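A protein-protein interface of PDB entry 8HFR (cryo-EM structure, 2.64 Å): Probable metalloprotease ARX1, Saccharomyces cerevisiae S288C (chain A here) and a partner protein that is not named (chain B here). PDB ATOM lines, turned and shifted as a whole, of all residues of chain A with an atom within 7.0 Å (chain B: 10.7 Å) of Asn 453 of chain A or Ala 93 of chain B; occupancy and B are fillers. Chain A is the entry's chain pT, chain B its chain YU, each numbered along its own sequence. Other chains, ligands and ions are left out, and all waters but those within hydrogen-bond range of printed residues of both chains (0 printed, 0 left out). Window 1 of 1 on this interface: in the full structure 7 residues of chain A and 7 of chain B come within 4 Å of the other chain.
O of Asn 453 of chain A lies within hydrogen-bond range of N of Ser 94 of chain B, at 2.9 Å.
Of the printed residues of chain B, Asn 453 of chain A touches Gly 92 (3.7 Å), Ala 93 (3.9 Å) and Ser 94 (2.9 Å).
Of chain B, only Ala 93 (3.3 Å) and Val 95 (3.97 Å) come within 4 Å of Pro 454 of chain A.
Of the printed residues of chain B, Asn 457 of chain A touches Asn 91 (3.2 Å).
No residue of chain B comes within 4 Å of Val 480 of chain A.
Printed residues of chain A within 4 Å of Asn 91 of chain B: Asn 457 (3.2 Å).
Of the printed residues of chain A, Gly 92 of chain B touches Asn 453 and Gly 456.
Ala 93 of chain B touches just these residues of chain A: Asn 453 (3.9 Å), Pro 454 (3.3 Å) and Gly 456 (3.4 Å).
Of the printed residues of chain A, Ser 94 of chain B touches Thr 452 and Asn 453.
Of the printed residues of chain A, Val 95 of chain B touches Pro 454.
Ile 97 of chain B touches none of the printed residues of chain A.
The nearest residue of chain A that does not touch Ala 93 of chain B is Asn 455 of chain A (4.1 Å).
Among the printed residues, pairs that only touch across the chains: Asn 457 of chain A with Asn 91 of chain B (3.2 Å), Pro 454 of chain A with Ala 93 of chain B (3.3 Å), Gly 456 of chain A with Ala 93 of chain B (3.4 Å), Thr 452 of chain A with Ser 94 of chain B (3.5 Å), Asn 453 of chain A with Gly 92 of chain B (3.7 Å), Asn 453 of chain A with Ala 93 of chain B (3.9 Å), Gly 456 of chain A with Gly 92 of chain B (3.95 Å) and Pro 454 of chain A with Val 95 of chain B (3.97 Å).
Printed residues of chain A that touch a printed residue of chain B: Thr 452, Asn 453, Pro 454, Gly 456 and Asn 457.
Hydrophobic or aromatic side chains of chain B within 4 Å of the printed part of chain A: Ala 93 and Val 95.
O of Val 95 of chain B is in hydrogen-bond range of N of Lys 87 of chain B (2.9 Å).
The side-chain amino group (NZ) of Lys 484 of chain A lies within hydrogen-bond range of the backbone carbonyl oxygen (O) of Thr 452 of chain A (3.1 Å).
The side-chain amide nitrogen of Asn 453 of chain A lies within hydrogen-bond range of the backbone carbonyl oxygen of Gly 479 of chain A (2.6 Å).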
ATOM      1  N   ALA A 451      19.988 -18.383 -19.827  1.00  0.00           N
ATOM      2  CA  ALA A 451      19.471 -19.043 -18.636  1.00  0.00           C
ATOM      3  C   ALA A 451      18.040 -19.515 -18.855  1.00  0.00           C
ATOM      4  O   ALA A 451      17.283 -18.925 -19.631  1.00  0.00           O
ATOM      5  CB  ALA A 451      19.554 -18.115 -17.427  1.00  0.00           C
ATOM      6  N   THR A 452      17.669 -20.595 -18.158  1.00  0.00           N
ATOM      7  CA  THR A 452      16.486 -21.384 -18.485  1.00  0.00           C
ATOM      8  C   THR A 452      15.557 -21.547 -17.286  1.00  0.00           C
ATOM      9  O   THR A 452      15.988 -21.507 -16.132  1.00  0.00           O
ATOM     10  CB  THR A 452      16.878 -22.778 -18.988  1.00  0.00           C
ATOM     11  OG1 THR A 452      17.634 -23.458 -17.976  1.00  0.00           O
ATOM     12  CG2 THR A 452      17.698 -22.689 -20.279  1.00  0.00           C
ATOM     13  N   ASN A 453      14.264 -21.773 -17.579  1.00  0.00           N
ATOM     14  CA  ASN A 453      13.232 -21.979 -16.575  1.00  0.00           C
ATOM     15  C   ASN A 453      12.628 -23.379 -16.654  1.00  0.00           C
ATOM     16  O   ASN A 453      12.363 -23.894 -17.741  1.00  0.00           O
ATOM     17  CB  ASN A 453      12.116 -20.932 -16.688  1.00  0.00           C
ATOM     18  CG  ASN A 453      11.631 -20.734 -18.099  1.00  0.00           C
ATOM     19  OD1 ASN A 453      12.089 -21.385 -19.031  1.00  0.00           O
ATOM     20  ND2 ASN A 453      10.697 -19.813 -18.268  1.00  0.00           N
ATOM     21  N   PRO A 454      12.405 -24.024 -15.510  1.00  0.00           N
ATOM     22  CA  PRO A 454      11.882 -25.396 -15.520  1.00  0.00           C
ATOM     23  C   PRO A 454      10.406 -25.484 -15.862  1.00  0.00           C
ATOM     24  O   PRO A 454       9.983 -26.426 -16.531  1.00  0.00           O
ATOM     25  CB  PRO A 454      12.146 -25.879 -14.089  1.00  0.00           C
ATOM     26  CG  PRO A 454      13.112 -24.892 -13.509  1.00  0.00           C
ATOM     27  CD  PRO A 454      12.796 -23.602 -14.160  1.00  0.00           C
ATOM     28  N   ASN A 455       9.609 -24.538 -15.384  1.00  0.00           N
ATOM     29  CA  ASN A 455       8.200 -24.420 -15.745  1.00  0.00           C
ATOM     30  C   ASN A 455       8.011 -23.060 -16.387  1.00  0.00           C
ATOM     31  O   ASN A 455       8.005 -22.041 -15.691  1.00  0.00           O
ATOM     32  CB  ASN A 455       7.292 -24.571 -14.529  1.00  0.00           C
ATOM     33  CG  ASN A 455       7.207 -25.987 -14.042  1.00  0.00           C
ATOM     34  OD1 ASN A 455       7.622 -26.296 -12.933  1.00  0.00           O
ATOM     35  ND2 ASN A 455       6.659 -26.862 -14.871  1.00  0.00           N
ATOM     36  N   GLY A 456       7.853 -23.041 -17.702  1.00  0.00           N
ATOM     37  CA  GLY A 456       7.883 -21.797 -18.435  1.00  0.00           C
ATOM     38  C   GLY A 456       6.663 -20.935 -18.237  1.00  0.00           C
ATOM     39  O   GLY A 456       6.742 -19.831 -17.691  1.00  0.00           O
ATOM     40  N   ASN A 457       5.521 -21.449 -18.660  1.00  0.00           N
ATOM     41  CA  ASN A 457       4.307 -20.660 -18.773  1.00  0.00           C
ATOM     42  C   ASN A 457       3.489 -20.643 -17.491  1.00  0.00           C
ATOM     43  O   ASN A 457       2.667 -19.744 -17.315  1.00  0.00           O
ATOM     44  CB  ASN A 457       3.453 -21.232 -19.905  1.00  0.00           C
ATOM     45  CG  ASN A 457       2.603 -20.211 -20.548  1.00  0.00           C
ATOM     46  OD1 ASN A 457       2.635 -19.051 -20.174  1.00  0.00           O
ATOM     47  ND2 ASN A 457       1.851 -20.620 -21.558  1.00  0.00           N
ATOM     48  N   SER A 459       4.447 -20.569 -14.154  1.00  0.00           N
ATOM     49  CA  SER A 459       4.955 -19.979 -12.928  1.00  0.00           C
ATOM     50  C   SER A 459       4.365 -18.593 -12.728  1.00  0.00           C
ATOM     51  O   SER A 459       4.216 -17.823 -13.679  1.00  0.00           O
ATOM     52  CB  SER A 459       6.480 -19.904 -12.953  1.00  0.00           C
ATOM     53  OG  SER A 459       6.938 -19.081 -14.006  1.00  0.00           O
ATOM     54  N   LEU A 478       8.007 -16.071 -25.357  1.00  0.00           N
ATOM     55  CA  LEU A 478       9.254 -16.704 -24.977  1.00  0.00           C
ATOM     56  C   LEU A 478       9.110 -17.571 -23.738  1.00  0.00           C
ATOM     57  O   LEU A 478       9.945 -18.452 -23.522  1.00  0.00           O
ATOM     58  CB  LEU A 478      10.335 -15.639 -24.739  1.00  0.00           C
ATOM     59  CG  LEU A 478      11.805 -16.010 -24.857  1.00  0.00           C
ATOM     60  CD1 LEU A 478      12.079 -16.662 -26.190  1.00  0.00           C
ATOM     61  CD2 LEU A 478      12.625 -14.750 -24.715  1.00  0.00           C
ATOM     62  N   GLY A 479       8.071 -17.356 -22.935  1.00  0.00           N
ATOM     63  CA  GLY A 479       7.758 -18.223 -21.820  1.00  0.00           C
ATOM     64  C   GLY A 479       8.418 -17.813 -20.524  1.00  0.00           C
ATOM     65  O   GLY A 479       8.825 -18.668 -19.734  1.00  0.00           O
ATOM     66  N   VAL A 480       8.536 -16.509 -20.293  1.00  0.00           N
ATOM     67  CA  VAL A 480       9.181 -15.968 -19.104  1.00  0.00           C
ATOM     68  C   VAL A 480       8.148 -15.168 -18.325  1.00  0.00           C
ATOM     69  O   VAL A 480       7.469 -14.307 -18.893  1.00  0.00           O
ATOM     70  CB  VAL A 480      10.400 -15.096 -19.465  1.00  0.00           C
ATOM     71  CG1 VAL A 480      11.124 -14.647 -18.216  1.00  0.00           C
ATOM     72  CG2 VAL A 480      11.346 -15.855 -20.374  1.00  0.00           C
ATOM     73  N   SER A 481       8.024 -15.459 -17.033  1.00  0.00           N
ATOM     74  CA  SER A 481       7.075 -14.792 -16.162  1.00  0.00           C
ATOM     75  C   SER A 481       7.788 -13.738 -15.317  1.00  0.00           C
ATOM     76  O   SER A 481       9.000 -13.534 -15.426  1.00  0.00           O
ATOM     77  CB  SER A 481       6.355 -15.820 -15.296  1.00  0.00           C
ATOM     78  OG  SER A 481       7.274 -16.725 -14.720  1.00  0.00           O
ATOM     79  N   LYS A 484      10.372 -15.161 -12.683  1.00  0.00           N
ATOM     80  CA  LYS A 484      11.582 -15.623 -13.344  1.00  0.00           C
ATOM     81  C   LYS A 484      12.399 -14.459 -13.880  1.00  0.00           C
ATOM     82  O   LYS A 484      13.631 -14.476 -13.802  1.00  0.00           O
ATOM     83  CB  LYS A 484      11.224 -16.594 -14.468  1.00  0.00           C
ATOM     84  CG  LYS A 484      12.418 -17.293 -15.071  1.00  0.00           C
ATOM     85  CD  LYS A 484      13.070 -18.195 -14.064  1.00  0.00           C
ATOM     86  CE  LYS A 484      14.326 -18.799 -14.624  1.00  0.00           C
ATOM     87  NZ  LYS A 484      14.820 -19.913 -13.783  1.00  0.00           N
ATOM     88  N   GLN B  81      25.991 -29.674 -15.859  1.00  0.00           N
ATOM     89  CA  GLN B  81      25.014 -29.026 -16.716  1.00  0.00           C
ATOM     90  C   GLN B  81      25.726 -27.986 -17.560  1.00  0.00           C
ATOM     91  O   GLN B  81      26.231 -26.986 -17.033  1.00  0.00           O
ATOM     92  CB  GLN B  81      23.894 -28.389 -15.900  1.00  0.00           C
ATOM     93  CG  GLN B  81      22.707 -29.294 -15.710  1.00  0.00           C
ATOM     94  CD  GLN B  81      21.937 -28.982 -14.455  1.00  0.00           C
ATOM     95  OE1 GLN B  81      21.796 -27.824 -14.075  1.00  0.00           O
ATOM     96  NE2 GLN B  81      21.426 -30.017 -13.807  1.00  0.00           N
ATOM     97  N   ASP B  83      25.496 -25.236 -20.616  1.00  0.00           N
ATOM     98  CA  ASP B  83      24.556 -24.317 -21.229  1.00  0.00           C
ATOM     99  C   ASP B  83      24.302 -24.717 -22.677  1.00  0.00           C
ATOM    100  O   ASP B  83      25.151 -25.336 -23.324  1.00  0.00           O
ATOM    101  CB  ASP B  83      25.116 -22.903 -21.165  1.00  0.00           C
ATOM    102  CG  ASP B  83      24.072 -21.879 -20.842  1.00  0.00           C
ATOM    103  OD1 ASP B  83      22.924 -22.281 -20.545  1.00  0.00           O
ATOM    104  OD2 ASP B  83      24.399 -20.675 -20.882  1.00  0.00           O
ATOM    105  N   VAL B  85      22.367 -26.974 -23.836  1.00  0.00           N
ATOM    106  CA  VAL B  85      22.032 -28.385 -24.028  1.00  0.00           C
ATOM    107  C   VAL B  85      20.847 -28.650 -23.102  1.00  0.00           C
ATOM    108  O   VAL B  85      21.014 -28.947 -21.917  1.00  0.00           O
ATOM    109  CB  VAL B  85      23.207 -29.326 -23.736  1.00  0.00           C
ATOM    110  CG1 VAL B  85      22.796 -30.785 -23.880  1.00  0.00           C
ATOM    111  CG2 VAL B  85      24.352 -29.047 -24.677  1.00  0.00           C
ATOM    112  N   THR B  86      19.637 -28.500 -23.631  1.00  0.00           N
ATOM    113  CA  THR B  86      18.422 -28.548 -22.832  1.00  0.00           C
ATOM    114  C   THR B  86      17.351 -29.322 -23.584  1.00  0.00           C
ATOM    115  O   THR B  86      17.422 -29.495 -24.801  1.00  0.00           O
ATOM    116  CB  THR B  86      17.882 -27.144 -22.515  1.00  0.00           C
ATOM    117  OG1 THR B  86      17.929 -26.335 -23.691  1.00  0.00           O
ATOM    118  CG2 THR B  86      18.672 -26.474 -21.411  1.00  0.00           C
ATOM    119  N   LYS B  87      16.348 -29.777 -22.846  1.00  0.00           N
ATOM    120  CA  LYS B  87      15.132 -30.312 -23.438  1.00  0.00           C
ATOM    121  C   LYS B  87      14.015 -29.293 -23.271  1.00  0.00           C
ATOM    122  O   LYS B  87      13.766 -28.818 -22.162  1.00  0.00           O
ATOM    123  CB  LYS B  87      14.738 -31.643 -22.802  1.00  0.00           C
ATOM    124  CG  LYS B  87      13.432 -32.184 -23.333  1.00  0.00           C
ATOM    125  CD  LYS B  87      13.193 -33.598 -22.881  1.00  0.00           C
ATOM    126  CE  LYS B  87      11.834 -34.081 -23.311  1.00  0.00           C
ATOM    127  NZ  LYS B  87      11.566 -35.413 -22.732  1.00  0.00           N
ATOM    128  N   GLU B  88      13.352 -28.963 -24.367  1.00  0.00           N
ATOM    129  CA  GLU B  88      12.337 -27.923 -24.379  1.00  0.00           C
ATOM    130  C   GLU B  88      10.942 -28.531 -24.408  1.00  0.00           C
ATOM    131  O   GLU B  88      10.749 -29.702 -24.737  1.00  0.00           O
ATOM    132  CB  GLU B  88      12.542 -26.997 -25.581  1.00  0.00           C
ATOM    133  CG  GLU B  88      11.852 -27.455 -26.853  1.00  0.00           C
ATOM    134  CD  GLU B  88      12.584 -28.578 -27.575  1.00  0.00           C
ATOM    135  OE1 GLU B  88      13.709 -28.945 -27.167  1.00  0.00           O
ATOM    136  OE2 GLU B  88      12.027 -29.104 -28.558  1.00  0.00           O
ATOM    137  N   LYS B  89       9.970 -27.720 -24.035  1.00  0.00           N
ATOM    138  CA  LYS B  89       8.577 -28.125 -24.026  1.00  0.00           C
ATOM    139  C   LYS B  89       7.779 -27.202 -24.936  1.00  0.00           C
ATOM    140  O   LYS B  89       8.301 -26.247 -25.506  1.00  0.00           O
ATOM    141  CB  LYS B  89       8.020 -28.121 -22.603  1.00  0.00           C
ATOM    142  CG  LYS B  89       8.764 -29.033 -21.660  1.00  0.00           C
ATOM    143  CD  LYS B  89       7.977 -29.253 -20.396  1.00  0.00           C
ATOM    144  CE  LYS B  89       8.807 -29.924 -19.336  1.00  0.00           C
ATOM    145  NZ  LYS B  89       8.091 -29.938 -18.043  1.00  0.00           N
ATOM    146  N   VAL B  90       6.493 -27.503 -25.072  1.00  0.00           N
ATOM    147  CA  VAL B  90       5.641 -26.737 -25.967  1.00  0.00           C
ATOM    148  C   VAL B  90       4.998 -25.544 -25.260  1.00  0.00           C
ATOM    149  O   VAL B  90       4.603 -24.575 -25.922  1.00  0.00           O
ATOM    150  CB  VAL B  90       4.617 -27.696 -26.604  1.00  0.00           C
ATOM    151  CG1 VAL B  90       3.594 -28.182 -25.580  1.00  0.00           C
ATOM    152  CG2 VAL B  90       3.959 -27.088 -27.844  1.00  0.00           C
ATOM    153  N   ASN B  91       4.939 -25.556 -23.933  1.00  0.00           N
ATOM    154  CA  ASN B  91       4.493 -24.396 -23.178  1.00  0.00           C
ATOM    155  C   ASN B  91       5.621 -23.418 -22.881  1.00  0.00           C
ATOM    156  O   ASN B  91       5.394 -22.432 -22.183  1.00  0.00           O
ATOM    157  CB  ASN B  91       3.829 -24.833 -21.870  1.00  0.00           C
ATOM    158  CG  ASN B  91       4.818 -25.348 -20.852  1.00  0.00           C
ATOM    159  OD1 ASN B  91       5.740 -26.086 -21.180  1.00  0.00           O
ATOM    160  ND2 ASN B  91       4.636 -24.952 -19.605  1.00  0.00           N
ATOM    161  N   GLY B  92       6.824 -23.654 -23.385  1.00  0.00           N
ATOM    162  CA  GLY B  92       7.905 -22.713 -23.216  1.00  0.00           C
ATOM    163  C   GLY B  92       8.901 -23.052 -22.138  1.00  0.00           C
ATOM    164  O   GLY B  92       9.793 -22.243 -21.868  1.00  0.00           O
ATOM    165  N   ALA B  93       8.781 -24.213 -21.516  1.00  0.00           N
ATOM    166  CA  ALA B  93       9.712 -24.626 -20.489  1.00  0.00           C
ATOM    167  C   ALA B  93      10.962 -25.226 -21.117  1.00  0.00           C
ATOM    168  O   ALA B  93      10.957 -25.679 -22.262  1.00  0.00           O
ATOM    169  CB  ALA B  93       9.051 -25.634 -19.562  1.00  0.00           C
ATOM    170  N   SER B  94      12.044 -25.235 -20.349  1.00  0.00           N
ATOM    171  CA  SER B  94      13.297 -25.812 -20.824  1.00  0.00           C
ATOM    172  C   SER B  94      14.044 -26.351 -19.617  1.00  0.00           C
ATOM    173  O   SER B  94      14.529 -25.571 -18.798  1.00  0.00           O
ATOM    174  CB  SER B  94      14.133 -24.783 -21.575  1.00  0.00           C
ATOM    175  OG  SER B  94      14.111 -23.530 -20.925  1.00  0.00           O
ATOM    176  N   VAL B  95      14.132 -27.672 -19.513  1.00  0.00           N
ATOM    177  CA  VAL B  95      14.853 -28.302 -18.410  1.00  0.00           C
ATOM    178  C   VAL B  95      16.258 -28.629 -18.900  1.00  0.00           C
ATOM    179  O   VAL B  95      16.452 -28.880 -20.094  1.00  0.00           O
ATOM    180  CB  VAL B  95      14.104 -29.541 -17.878  1.00  0.00           C
ATOM    181  CG1 VAL B  95      12.737 -29.151 -17.381  1.00  0.00           C
ATOM    182  CG2 VAL B  95      13.961 -30.612 -18.933  1.00  0.00           C
ATOM    183  N   PRO B  96      17.273 -28.580 -18.045  1.00  0.00           N
ATOM    184  CA  PRO B  96      18.622 -28.939 -18.488  1.00  0.00           C
ATOM    185  C   PRO B  96      18.848 -30.442 -18.453  1.00  0.00           C
ATOM    186  O   PRO B  96      18.233 -31.172 -17.673  1.00  0.00           O
ATOM    187  CB  PRO B  96      19.534 -28.220 -17.482  1.00  0.00           C
ATOM    188  CG  PRO B  96      18.621 -27.397 -16.601  1.00  0.00           C
ATOM    189  CD  PRO B  96      17.276 -28.015 -16.688  1.00  0.00           C
ATOM    190  N   ILE B  97      19.744 -30.897 -19.323  1.00  0.00           N
ATOM    191  CA  ILE B  97      20.114 -32.303 -19.409  1.00  0.00           C
ATOM    192  C   ILE B  97      21.266 -32.560 -18.446  1.00  0.00           C
ATOM    193  O   ILE B  97      22.239 -31.799 -18.415  1.00  0.00           O
ATOM    194  CB  ILE B  97      20.506 -32.677 -20.847  1.00  0.00           C
ATOM    195  CG1 ILE B  97      19.368 -32.382 -21.828  1.00  0.00           C
ATOM    196  CG2 ILE B  97      20.953 -34.128 -20.938  1.00  0.00           C
ATOM    197  CD1 ILE B  97      18.273 -33.395 -21.850  1.00  0.00           C
